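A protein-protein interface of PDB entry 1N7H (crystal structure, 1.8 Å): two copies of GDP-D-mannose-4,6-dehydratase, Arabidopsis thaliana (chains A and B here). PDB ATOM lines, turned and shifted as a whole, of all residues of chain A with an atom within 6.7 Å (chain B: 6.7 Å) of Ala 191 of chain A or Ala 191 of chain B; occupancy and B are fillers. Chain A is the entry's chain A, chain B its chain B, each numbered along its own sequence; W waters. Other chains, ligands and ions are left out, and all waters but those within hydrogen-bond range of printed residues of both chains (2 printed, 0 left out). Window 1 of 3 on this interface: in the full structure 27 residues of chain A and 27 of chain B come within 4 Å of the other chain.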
ATOM      1  N   VAL A 133     -22.253  24.776   4.963  1.00  0.00           N
ATOM      2  CA  VAL A 133     -22.898  23.614   4.361  1.00  0.00           C
ATOM      3  C   VAL A 133     -21.967  22.472   3.964  1.00  0.00           C
ATOM      4  O   VAL A 133     -22.314  21.301   4.119  1.00  0.00           O
ATOM      5  CB  VAL A 133     -23.742  24.083   3.146  1.00  0.00           C
ATOM      6  CG1 VAL A 133     -24.451  22.896   2.475  1.00  0.00           C
ATOM      7  CG2 VAL A 133     -24.791  25.091   3.626  1.00  0.00           C
ATOM      8  N   ALA A 134     -20.780  22.805   3.473  1.00  0.00           N
ATOM      9  CA  ALA A 134     -19.838  21.773   3.066  1.00  0.00           C
ATOM     10  C   ALA A 134     -18.821  21.495   4.169  1.00  0.00           C
ATOM     11  O   ALA A 134     -18.834  20.433   4.790  1.00  0.00           O
ATOM     12  CB  ALA A 134     -19.128  22.189   1.782  1.00  0.00           C
ATOM     13  N   THR A 135     -17.944  22.455   4.432  1.00  0.00           N
ATOM     14  CA  THR A 135     -16.933  22.230   5.451  1.00  0.00           C
ATOM     15  C   THR A 135     -17.517  22.058   6.856  1.00  0.00           C
ATOM     16  O   THR A 135     -17.002  21.266   7.642  1.00  0.00           O
ATOM     17  CB  THR A 135     -15.887  23.359   5.425  1.00  0.00           C
ATOM     18  OG1 THR A 135     -15.412  23.515   4.083  1.00  0.00           O
ATOM     19  CG2 THR A 135     -14.701  23.005   6.313  1.00  0.00           C
ATOM     20  N   ALA A 137     -20.180  20.576   7.726  1.00  0.00           N
ATOM     21  CA  ALA A 137     -20.616  19.188   7.879  1.00  0.00           C
ATOM     22  C   ALA A 137     -19.391  18.326   8.191  1.00  0.00           C
ATOM     23  O   ALA A 137     -19.441  17.458   9.064  1.00  0.00           O
ATOM     24  CB  ALA A 137     -21.300  18.704   6.590  1.00  0.00           C
ATOM     25  N   MET A 165     -29.218  18.654  -4.794  1.00  0.00           N
ATOM     26  CA  MET A 165     -27.972  18.069  -5.276  1.00  0.00           C
ATOM     27  C   MET A 165     -28.103  17.546  -6.705  1.00  0.00           C
ATOM     28  O   MET A 165     -27.141  17.582  -7.472  1.00  0.00           O
ATOM     29  CB  MET A 165     -27.512  16.945  -4.341  1.00  0.00           C
ATOM     30  CG  MET A 165     -27.189  17.441  -2.930  1.00  0.00           C
ATOM     31  SD  MET A 165     -26.594  16.142  -1.808  1.00  0.00           S
ATOM     32  CE  MET A 165     -27.884  14.902  -1.992  1.00  0.00           C
ATOM     33  N   PHE A 179     -25.496  13.735  -9.727  1.00  0.00           N
ATOM     34  CA  PHE A 179     -25.662  15.102  -9.252  1.00  0.00           C
ATOM     35  C   PHE A 179     -25.153  16.086 -10.304  1.00  0.00           C
ATOM     36  O   PHE A 179     -24.101  15.866 -10.903  1.00  0.00           O
ATOM     37  CB  PHE A 179     -24.825  15.382  -7.996  1.00  0.00           C
ATOM     38  CG  PHE A 179     -25.164  14.542  -6.795  1.00  0.00           C
ATOM     39  CD1 PHE A 179     -26.439  14.016  -6.607  1.00  0.00           C
ATOM     40  CD2 PHE A 179     -24.207  14.355  -5.795  1.00  0.00           C
ATOM     41  CE1 PHE A 179     -26.756  13.317  -5.434  1.00  0.00           C
ATOM     42  CE2 PHE A 179     -24.514  13.660  -4.618  1.00  0.00           C
ATOM     43  CZ  PHE A 179     -25.797  13.140  -4.441  1.00  0.00           C
ATOM     44  N   ALA A 186     -26.189  24.039  -3.591  1.00  0.00           N
ATOM     45  CA  ALA A 186     -26.323  22.668  -4.079  1.00  0.00           C
ATOM     46  C   ALA A 186     -24.986  21.946  -4.134  1.00  0.00           C
ATOM     47  O   ALA A 186     -24.880  20.787  -3.724  1.00  0.00           O
ATOM     48  CB  ALA A 186     -26.990  22.668  -5.461  1.00  0.00           C
ATOM     49  N   ALA A 187     -23.965  22.635  -4.638  1.00  0.00           N
ATOM     50  CA  ALA A 187     -22.641  22.043  -4.751  1.00  0.00           C
ATOM     51  C   ALA A 187     -22.083  21.730  -3.368  1.00  0.00           C
ATOM     52  O   ALA A 187     -21.427  20.705  -3.171  1.00  0.00           O
ATOM     53  CB  ALA A 187     -21.706  22.990  -5.499  1.00  0.00           C
ATOM     54  N   SER A 188     -22.360  22.609  -2.411  1.00  0.00           N
ATOM     55  CA  SER A 188     -21.881  22.412  -1.048  1.00  0.00           C
ATOM     56  C   SER A 188     -22.593  21.223  -0.410  1.00  0.00           C
ATOM     57  O   SER A 188     -21.984  20.483   0.364  1.00  0.00           O
ATOM     58  CB  SER A 188     -22.094  23.685  -0.225  1.00  0.00           C
ATOM     59  OG  SER A 188     -21.294  24.747  -0.739  1.00  0.00           O
ATOM     60  N   LYS A 189     -23.876  21.032  -0.714  1.00  0.00           N
ATOM     61  CA  LYS A 189     -24.580  19.873  -0.155  1.00  0.00           C
ATOM     62  C   LYS A 189     -23.995  18.597  -0.762  1.00  0.00           C
ATOM     63  O   LYS A 189     -23.876  17.571  -0.081  1.00  0.00           O
ATOM     64  CB  LYS A 189     -26.091  19.948  -0.417  1.00  0.00           C
ATOM     65  CG  LYS A 189     -26.850  20.844   0.590  1.00  0.00           C
ATOM     66  CD  LYS A 189     -26.825  20.252   2.004  1.00  0.00           C
ATOM     67  CE  LYS A 189     -27.698  21.063   2.950  1.00  0.00           C
ATOM     68  NZ  LYS A 189     -27.717  20.502   4.347  1.00  0.00           N
ATOM     69  N   CYS A 190     -23.635  18.654  -2.044  1.00  0.00           N
ATOM     70  CA  CYS A 190     -23.028  17.493  -2.693  1.00  0.00           C
ATOM     71  C   CYS A 190     -21.745  17.153  -1.949  1.00  0.00           C
ATOM     72  O   CYS A 190     -21.446  15.976  -1.713  1.00  0.00           O
ATOM     73  CB  CYS A 190     -22.683  17.790  -4.153  1.00  0.00           C
ATOM     74  SG  CYS A 190     -24.119  17.896  -5.250  1.00  0.00           S
ATOM     75  N   ALA A 191     -20.980  18.184  -1.594  1.00  0.00           N
ATOM     76  CA  ALA A 191     -19.735  17.972  -0.863  1.00  0.00           C
ATOM     77  C   ALA A 191     -20.022  17.292   0.479  1.00  0.00           C
ATOM     78  O   ALA A 191     -19.384  16.299   0.813  1.00  0.00           O
ATOM     79  CB  ALA A 191     -19.014  19.315  -0.637  1.00  0.00           C
ATOM     80  N   ALA A 192     -20.986  17.827   1.232  1.00  0.00           N
ATOM     81  CA  ALA A 192     -21.344  17.263   2.538  1.00  0.00           C
ATOM     82  C   ALA A 192     -21.788  15.808   2.383  1.00  0.00           C
ATOM     83  O   ALA A 192     -21.502  14.963   3.231  1.00  0.00           O
ATOM     84  CB  ALA A 192     -22.467  18.090   3.193  1.00  0.00           C
ATOM     85  N   HIS A 193     -22.507  15.532   1.304  1.00  0.00           N
ATOM     86  CA  HIS A 193     -22.986  14.178   1.038  1.00  0.00           C
ATOM     87  C   HIS A 193     -21.797  13.232   0.928  1.00  0.00           C
ATOM     88  O   HIS A 193     -21.752  12.189   1.583  1.00  0.00           O
ATOM     89  CB  HIS A 193     -23.769  14.153  -0.277  1.00  0.00           C
ATOM     90  CG  HIS A 193     -24.315  12.805  -0.633  1.00  0.00           C
ATOM     91  ND1 HIS A 193     -25.524  12.342  -0.161  1.00  0.00           N
ATOM     92  CD2 HIS A 193     -23.818  11.825  -1.424  1.00  0.00           C
ATOM     93  CE1 HIS A 193     -25.751  11.135  -0.649  1.00  0.00           C
ATOM     94  NE2 HIS A 193     -24.731  10.798  -1.418  1.00  0.00           N
ATOM     95  N   TRP A 194     -20.833  13.598   0.091  1.00  0.00           N
ATOM     96  CA  TRP A 194     -19.667  12.758  -0.099  1.00  0.00           C
ATOM     97  C   TRP A 194     -18.744  12.676   1.115  1.00  0.00           C
ATOM     98  O   TRP A 194     -18.126  11.635   1.338  1.00  0.00           O
ATOM     99  CB  TRP A 194     -18.932  13.155  -1.375  1.00  0.00           C
ATOM    100  CG  TRP A 194     -19.685  12.607  -2.556  1.00  0.00           C
ATOM    101  CD1 TRP A 194     -20.388  13.315  -3.485  1.00  0.00           C
ATOM    102  CD2 TRP A 194     -19.904  11.219  -2.859  1.00  0.00           C
ATOM    103  NE1 TRP A 194     -21.038  12.458  -4.346  1.00  0.00           N
ATOM    104  CE2 TRP A 194     -20.756  11.166  -3.984  1.00  0.00           C
ATOM    105  CE3 TRP A 194     -19.465  10.017  -2.286  1.00  0.00           C
ATOM    106  CZ2 TRP A 194     -21.179   9.952  -4.552  1.00  0.00           C
ATOM    107  CZ3 TRP A 194     -19.888   8.808  -2.850  1.00  0.00           C
ATOM    108  CH2 TRP A 194     -20.734   8.790  -3.969  1.00  0.00           C
ATOM    109  N   TYR A 195     -18.647  13.740   1.908  1.00  0.00           N
ATOM    110  CA  TYR A 195     -17.824  13.677   3.124  1.00  0.00           C
ATOM    111  C   TYR A 195     -18.475  12.651   4.059  1.00  0.00           C
ATOM    112  O   TYR A 195     -17.799  11.869   4.729  1.00  0.00           O
ATOM    113  CB  TYR A 195     -17.794  15.032   3.847  1.00  0.00           C
ATOM    114  CG  TYR A 195     -17.009  16.128   3.152  1.00  0.00           C
ATOM    115  CD1 TYR A 195     -17.454  17.445   3.192  1.00  0.00           C
ATOM    116  CD2 TYR A 195     -15.813  15.854   2.481  1.00  0.00           C
ATOM    117  CE1 TYR A 195     -16.739  18.471   2.582  1.00  0.00           C
ATOM    118  CE2 TYR A 195     -15.083  16.878   1.866  1.00  0.00           C
ATOM    119  CZ  TYR A 195     -15.558  18.182   1.921  1.00  0.00           C
ATOM    120  OH  TYR A 195     -14.869  19.200   1.302  1.00  0.00           O
ATOM    121  N   THR A 196     -19.802  12.662   4.096  1.00  0.00           N
ATOM    122  CA  THR A 196     -20.557  11.756   4.960  1.00  0.00           C
ATOM    123  C   THR A 196     -20.430  10.299   4.494  1.00  0.00           C
ATOM    124  O   THR A 196     -20.193   9.399   5.307  1.00  0.00           O
ATOM    125  CB  THR A 196     -22.028  12.210   5.019  1.00  0.00           C
ATOM    126  OG1 THR A 196     -22.069  13.564   5.494  1.00  0.00           O
ATOM    127  CG2 THR A 196     -22.838  11.339   5.972  1.00  0.00           C
ATOM    128  N   VAL B 133      -8.871  22.945  -0.714  1.00  0.00           N
ATOM    129  CA  VAL B 133      -9.239  22.270  -1.956  1.00  0.00           C
ATOM    130  C   VAL B 133     -10.656  22.518  -2.451  1.00  0.00           C
ATOM    131  O   VAL B 133     -10.881  22.620  -3.656  1.00  0.00           O
ATOM    132  CB  VAL B 133      -8.982  20.744  -1.802  1.00  0.00           C
ATOM    133  CG1 VAL B 133      -9.372  19.983  -3.073  1.00  0.00           C
ATOM    134  CG2 VAL B 133      -7.491  20.521  -1.513  1.00  0.00           C
ATOM    135  N   ALA B 134     -11.606  22.629  -1.530  1.00  0.00           N
ATOM    136  CA  ALA B 134     -12.986  22.873  -1.927  1.00  0.00           C
ATOM    137  C   ALA B 134     -13.332  24.357  -1.826  1.00  0.00           C
ATOM    138  O   ALA B 134     -13.547  25.024  -2.839  1.00  0.00           O
ATOM    139  CB  ALA B 134     -13.939  22.048  -1.058  1.00  0.00           C
ATOM    140  N   THR B 135     -13.379  24.883  -0.606  1.00  0.00           N
ATOM    141  CA  THR B 135     -13.741  26.285  -0.442  1.00  0.00           C
ATOM    142  C   THR B 135     -12.720  27.243  -1.049  1.00  0.00           C
ATOM    143  O   THR B 135     -13.096  28.282  -1.589  1.00  0.00           O
ATOM    144  CB  THR B 135     -13.978  26.624   1.034  1.00  0.00           C
ATOM    145  OG1 THR B 135     -14.896  25.671   1.583  1.00  0.00           O
ATOM    146  CG2 THR B 135     -14.593  28.032   1.169  1.00  0.00           C
ATOM    147  N   ALA B 137     -11.067  26.929  -3.730  1.00  0.00           N
ATOM    148  CA  ALA B 137     -11.334  27.042  -5.164  1.00  0.00           C
ATOM    149  C   ALA B 137     -12.492  28.015  -5.375  1.00  0.00           C
ATOM    150  O   ALA B 137     -12.454  28.859  -6.275  1.00  0.00           O
ATOM    151  CB  ALA B 137     -11.681  25.665  -5.752  1.00  0.00           C
ATOM    152  N   MET B 165     -11.424  12.006  -8.079  1.00  0.00           N
ATOM    153  CA  MET B 165     -12.851  12.265  -7.931  1.00  0.00           C
ATOM    154  C   MET B 165     -13.690  11.032  -8.274  1.00  0.00           C
ATOM    155  O   MET B 165     -14.764  10.830  -7.702  1.00  0.00           O
ATOM    156  CB  MET B 165     -13.275  13.449  -8.814  1.00  0.00           C
ATOM    157  CG  MET B 165     -12.585  14.748  -8.439  1.00  0.00           C
ATOM    158  SD  MET B 165     -13.124  16.189  -9.407  1.00  0.00           S
ATOM    159  CE  MET B 165     -12.878  15.594 -11.104  1.00  0.00           C
ATOM    160  N   PHE B 179     -18.872  10.187  -9.997  1.00  0.00           N
ATOM    161  CA  PHE B 179     -17.875  10.323  -8.942  1.00  0.00           C
ATOM    162  C   PHE B 179     -18.294   9.525  -7.714  1.00  0.00           C
ATOM    163  O   PHE B 179     -19.461   9.541  -7.332  1.00  0.00           O
ATOM    164  CB  PHE B 179     -17.746  11.780  -8.463  1.00  0.00           C
ATOM    165  CG  PHE B 179     -17.324  12.764  -9.517  1.00  0.00           C
ATOM    166  CD1 PHE B 179     -16.521  12.387 -10.588  1.00  0.00           C
ATOM    167  CD2 PHE B 179     -17.665  14.106  -9.374  1.00  0.00           C
ATOM    168  CE1 PHE B 179     -16.061  13.346 -11.502  1.00  0.00           C
ATOM    169  CE2 PHE B 179     -17.212  15.068 -10.273  1.00  0.00           C
ATOM    170  CZ  PHE B 179     -16.406  14.685 -11.341  1.00  0.00           C
ATOM    171  N   ALA B 186     -10.496  13.773  -2.187  1.00  0.00           N
ATOM    172  CA  ALA B 186     -11.300  13.483  -3.369  1.00  0.00           C
ATOM    173  C   ALA B 186     -12.662  14.171  -3.326  1.00  0.00           C
ATOM    174  O   ALA B 186     -13.109  14.740  -4.326  1.00  0.00           O
ATOM    175  CB  ALA B 186     -11.473  11.964  -3.523  1.00  0.00           C
ATOM    176  N   ALA B 187     -13.322  14.115  -2.174  1.00  0.00           N
ATOM    177  CA  ALA B 187     -14.633  14.749  -2.031  1.00  0.00           C
ATOM    178  C   ALA B 187     -14.488  16.260  -2.208  1.00  0.00           C
ATOM    179  O   ALA B 187     -15.350  16.928  -2.799  1.00  0.00           O
ATOM    180  CB  ALA B 187     -15.225  14.433  -0.661  1.00  0.00           C
ATOM    181  N   SER B 188     -13.396  16.808  -1.693  1.00  0.00           N
ATOM    182  CA  SER B 188     -13.170  18.242  -1.826  1.00  0.00           C
ATOM    183  C   SER B 188     -12.916  18.622  -3.280  1.00  0.00           C
ATOM    184  O   SER B 188     -13.346  19.686  -3.716  1.00  0.00           O
ATOM    185  CB  SER B 188     -12.003  18.680  -0.938  1.00  0.00           C
ATOM    186  OG  SER B 188     -12.338  18.466   0.433  1.00  0.00           O
ATOM    187  N   LYS B 189     -12.219  17.771  -4.030  1.00  0.00           N
ATOM    188  CA  LYS B 189     -11.988  18.074  -5.448  1.00  0.00           C
ATOM    189  C   LYS B 189     -13.314  18.005  -6.199  1.00  0.00           C
ATOM    190  O   LYS B 189     -13.539  18.767  -7.137  1.00  0.00           O
ATOM    191  CB  LYS B 189     -10.977  17.105  -6.071  1.00  0.00           C
ATOM    192  CG  LYS B 189      -9.503  17.477  -5.779  1.00  0.00           C
ATOM    193  CD  LYS B 189      -9.104  18.765  -6.486  1.00  0.00           C
ATOM    194  CE  LYS B 189      -7.622  19.079  -6.291  1.00  0.00           C
ATOM    195  NZ  LYS B 189      -7.245  20.348  -6.997  1.00  0.00           N
ATOM    196  N   CYS B 190     -14.191  17.089  -5.792  1.00  0.00           N
ATOM    197  CA  CYS B 190     -15.502  16.972  -6.418  1.00  0.00           C
ATOM    198  C   CYS B 190     -16.251  18.282  -6.192  1.00  0.00           C
ATOM    199  O   CYS B 190     -16.913  18.807  -7.098  1.00  0.00           O
ATOM    200  CB  CYS B 190     -16.305  15.819  -5.807  1.00  0.00           C
ATOM    201  SG  CYS B 190     -15.739  14.161  -6.272  1.00  0.00           S
ATOM    202  N   ALA B 191     -16.139  18.814  -4.978  1.00  0.00           N
ATOM    203  CA  ALA B 191     -16.786  20.080  -4.648  1.00  0.00           C
ATOM    204  C   ALA B 191     -16.250  21.192  -5.557  1.00  0.00           C
ATOM    205  O   ALA B 191     -17.029  21.933  -6.170  1.00  0.00           O
ATOM    206  CB  ALA B 191     -16.541  20.436  -3.171  1.00  0.00           C
ATOM    207  N   ALA B 192     -14.925  21.305  -5.648  1.00  0.00           N
ATOM    208  CA  ALA B 192     -14.304  22.332  -6.493  1.00  0.00           C
ATOM    209  C   ALA B 192     -14.758  22.196  -7.944  1.00  0.00           C
ATOM    210  O   ALA B 192     -14.965  23.195  -8.637  1.00  0.00           O
ATOM    211  CB  ALA B 192     -12.757  22.234  -6.421  1.00  0.00           C
ATOM    212  N   HIS B 193     -14.894  20.953  -8.402  1.00  0.00           N
ATOM    213  CA  HIS B 193     -15.324  20.677  -9.770  1.00  0.00           C
ATOM    214  C   HIS B 193     -16.706  21.285  -9.985  1.00  0.00           C
ATOM    215  O   HIS B 193     -16.934  22.026 -10.941  1.00  0.00           O
ATOM    216  CB  HIS B 193     -15.404  19.161  -9.998  1.00  0.00           C
ATOM    217  CG  HIS B 193     -15.815  18.774 -11.387  1.00  0.00           C
ATOM    218  ND1 HIS B 193     -14.911  18.622 -12.417  1.00  0.00           N
ATOM    219  CD2 HIS B 193     -17.034  18.510 -11.915  1.00  0.00           C
ATOM    220  CE1 HIS B 193     -15.557  18.286 -13.521  1.00  0.00           C
ATOM    221  NE2 HIS B 193     -16.846  18.212 -13.244  1.00  0.00           N
ATOM    222  N   TRP B 194     -17.630  20.962  -9.085  1.00  0.00           N
ATOM    223  CA  TRP B 194     -18.984  21.475  -9.201  1.00  0.00           C
ATOM    224  C   TRP B 194     -19.100  22.983  -9.000  1.00  0.00           C
ATOM    225  O   TRP B 194     -19.917  23.624  -9.652  1.00  0.00           O
ATOM    226  CB  TRP B 194     -19.895  20.753  -8.202  1.00  0.00           C
ATOM    227  CG  TRP B 194     -20.014  19.278  -8.461  1.00  0.00           C
ATOM    228  CD1 TRP B 194     -20.243  18.675  -9.667  1.00  0.00           C
ATOM    229  CD2 TRP B 194     -19.955  18.221  -7.491  1.00  0.00           C
ATOM    230  NE1 TRP B 194     -20.331  17.314  -9.509  1.00  0.00           N
ATOM    231  CE2 TRP B 194     -20.162  17.006  -8.185  1.00  0.00           C
ATOM    232  CE3 TRP B 194     -19.749  18.183  -6.105  1.00  0.00           C
ATOM    233  CZ2 TRP B 194     -20.171  15.767  -7.539  1.00  0.00           C
ATOM    234  CZ3 TRP B 194     -19.756  16.948  -5.464  1.00  0.00           C
ATOM    235  CH2 TRP B 194     -19.968  15.759  -6.183  1.00  0.00           C
ATOM    236  N   TYR B 195     -18.276  23.573  -8.136  1.00  0.00           N
ATOM    237  CA  TYR B 195     -18.328  25.028  -7.974  1.00  0.00           C
ATOM    238  C   TYR B 195     -17.895  25.663  -9.301  1.00  0.00           C
ATOM    239  O   TYR B 195     -18.449  26.679  -9.735  1.00  0.00           O
ATOM    240  CB  TYR B 195     -17.355  25.508  -6.889  1.00  0.00           C
ATOM    241  CG  TYR B 195     -17.734  25.140  -5.467  1.00  0.00           C
ATOM    242  CD1 TYR B 195     -16.753  24.757  -4.550  1.00  0.00           C
ATOM    243  CD2 TYR B 195     -19.060  25.190  -5.033  1.00  0.00           C
ATOM    244  CE1 TYR B 195     -17.076  24.423  -3.237  1.00  0.00           C
ATOM    245  CE2 TYR B 195     -19.399  24.860  -3.712  1.00  0.00           C
ATOM    246  CZ  TYR B 195     -18.399  24.474  -2.825  1.00  0.00           C
ATOM    247  OH  TYR B 195     -18.720  24.120  -1.527  1.00  0.00           O
ATOM    248  N   THR B 196     -16.896  25.057  -9.932  1.00  0.00           N
ATOM    249  CA  THR B 196     -16.361  25.578 -11.194  1.00  0.00           C
ATOM    250  C   THR B 196     -17.384  25.449 -12.329  1.00  0.00           C
ATOM    251  O   THR B 196     -17.612  26.408 -13.079  1.00  0.00           O
ATOM    252  CB  THR B 196     -15.037  24.866 -11.537  1.00  0.00           C
ATOM    253  OG1 THR B 196     -14.124  25.048 -10.446  1.00  0.00           O
ATOM    254  CG2 THR B 196     -14.394  25.447 -12.805  1.00  0.00           C
HETATM  255  O   HOH W   1     -21.283  14.704 -10.276  1.00  0.00           O
HETATM  256  O   HOH W   2     -14.373  26.023   4.248  1.00  0.00           O
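Of the 17 printed residues of chain A, 8 touch a printed residue of chain B.
Printed residues of chain A that touch a printed residue of chain B: Ala 134, Thr 135, Ala 187, Ser 188, Cys 190, Ala 191, Trp 194 and Tyr 195.
Along chain A the printed residues that touch a printed residue of chain B span positions 134 to 195.
Among the printed residues, no Asp or Glu carboxylate lies within 4 Å of a Lys or Arg side-chain nitrogen of the other chain.
Ala 191 of chain A touches just one residue of chain B: Ala 191.
Ala 191 of chain B touches just one residue of chain A: Ala 191.
Printed residues of chain A within 4 Å of Ala 187 of chain B: Trp 194 and Tyr 195.
Printed residues of chain A within 4 Å of Tyr 195 of chain B: Ala 134, Ala 187 and Ser 188.
Of the printed residues of chain B, Cys 190 of chain A touches Trp 194.
Of the printed residues of chain B, Tyr 195 of chain A touches Ala 134, Ala 187 and Ser 188.
Of the printed residues of chain B, Trp 194 of chain A touches Phe 179, Ala 187 and Trp 194.
His 193 of chain A touches none of the printed residues of chain B.
Met 165 of chain A touches none of the printed residues of chain B.
Among the printed residues, pairs that only touch across the chains: Trp 194 of chain A with Phe 179 of chain B, Cys 190 of chain A with Trp 194 of chain B, Ala 187 of chain A with Tyr 195 of chain B, Tyr 195 of chain A with Ala 187 of chain B, Trp 194 of chain A with Trp 194 of chain B, Ala 191 of chain A with Ala 191 of chain B, Tyr 195 of chain A with Ala 134 of chain B, Ala 134 of chain A with Tyr 195 of chain B, Ala 187 of chain A with Trp 194 of chain B and Trp 194 of chain A with Ala 187 of chain B.
The backbone carbonyl oxygen (O) of Met 165 of chain A sits close to the side-chain sulfur (SG) of Cys 190 of chain A (3.8 Å).
The backbone carbonyl oxygen (O) of Ala 186 of chain A is in hydrogen-bond range of the side-chain sulfur (SG) of Cys 190 of chain A (3.4 Å).
Water W2 bridges the side-chain hydroxyl (OG1) of Thr 135 of chain A (2.7 Å) and the side-chain hydroxyl (OG1) of Thr 135 of chain B (2.7 Å).
Water W1 lies within hydrogen-bond range of the indole nitrogen (NE1) of Trp 194 of chain B and the backbone carbonyl oxygen (O) of Phe 179 of chain A.
The side-chain hydroxyl (OG1) of Thr 135 of chain A is in hydrogen-bond range of the side-chain hydroxyl (OG1) of Thr 135 of chain B, at 3.3 Å.
OG of Ser 188 of chain A is in hydrogen-bond range of OH of Tyr 195 of chain B (2.8 Å).
OH of Tyr 195 of chain A sits at hydrogen-bond distance from OG of Ser 188 of chain B, at 2.8 Å.
Ala 134 of chain A touches Tyr 195 of chain B, and with the chains exchanged Tyr 195 of chain A touches Ala 134 of chain B.
Ala 187 of chain A touches Trp 194 of chain B, and with the chains exchanged Trp 194 of chain A touches Ala 187 of chain B.
Ala 187 of chain A touches Tyr 195 of chain B, and with the chains exchanged Tyr 195 of chain A touches Ala 187 of chain B.
Ser 188 of chain A touches Tyr 195 of chain B, and with the chains exchanged Tyr 195 of chain A touches Ser 188 of chain B.
17 positions are printed for both chains.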
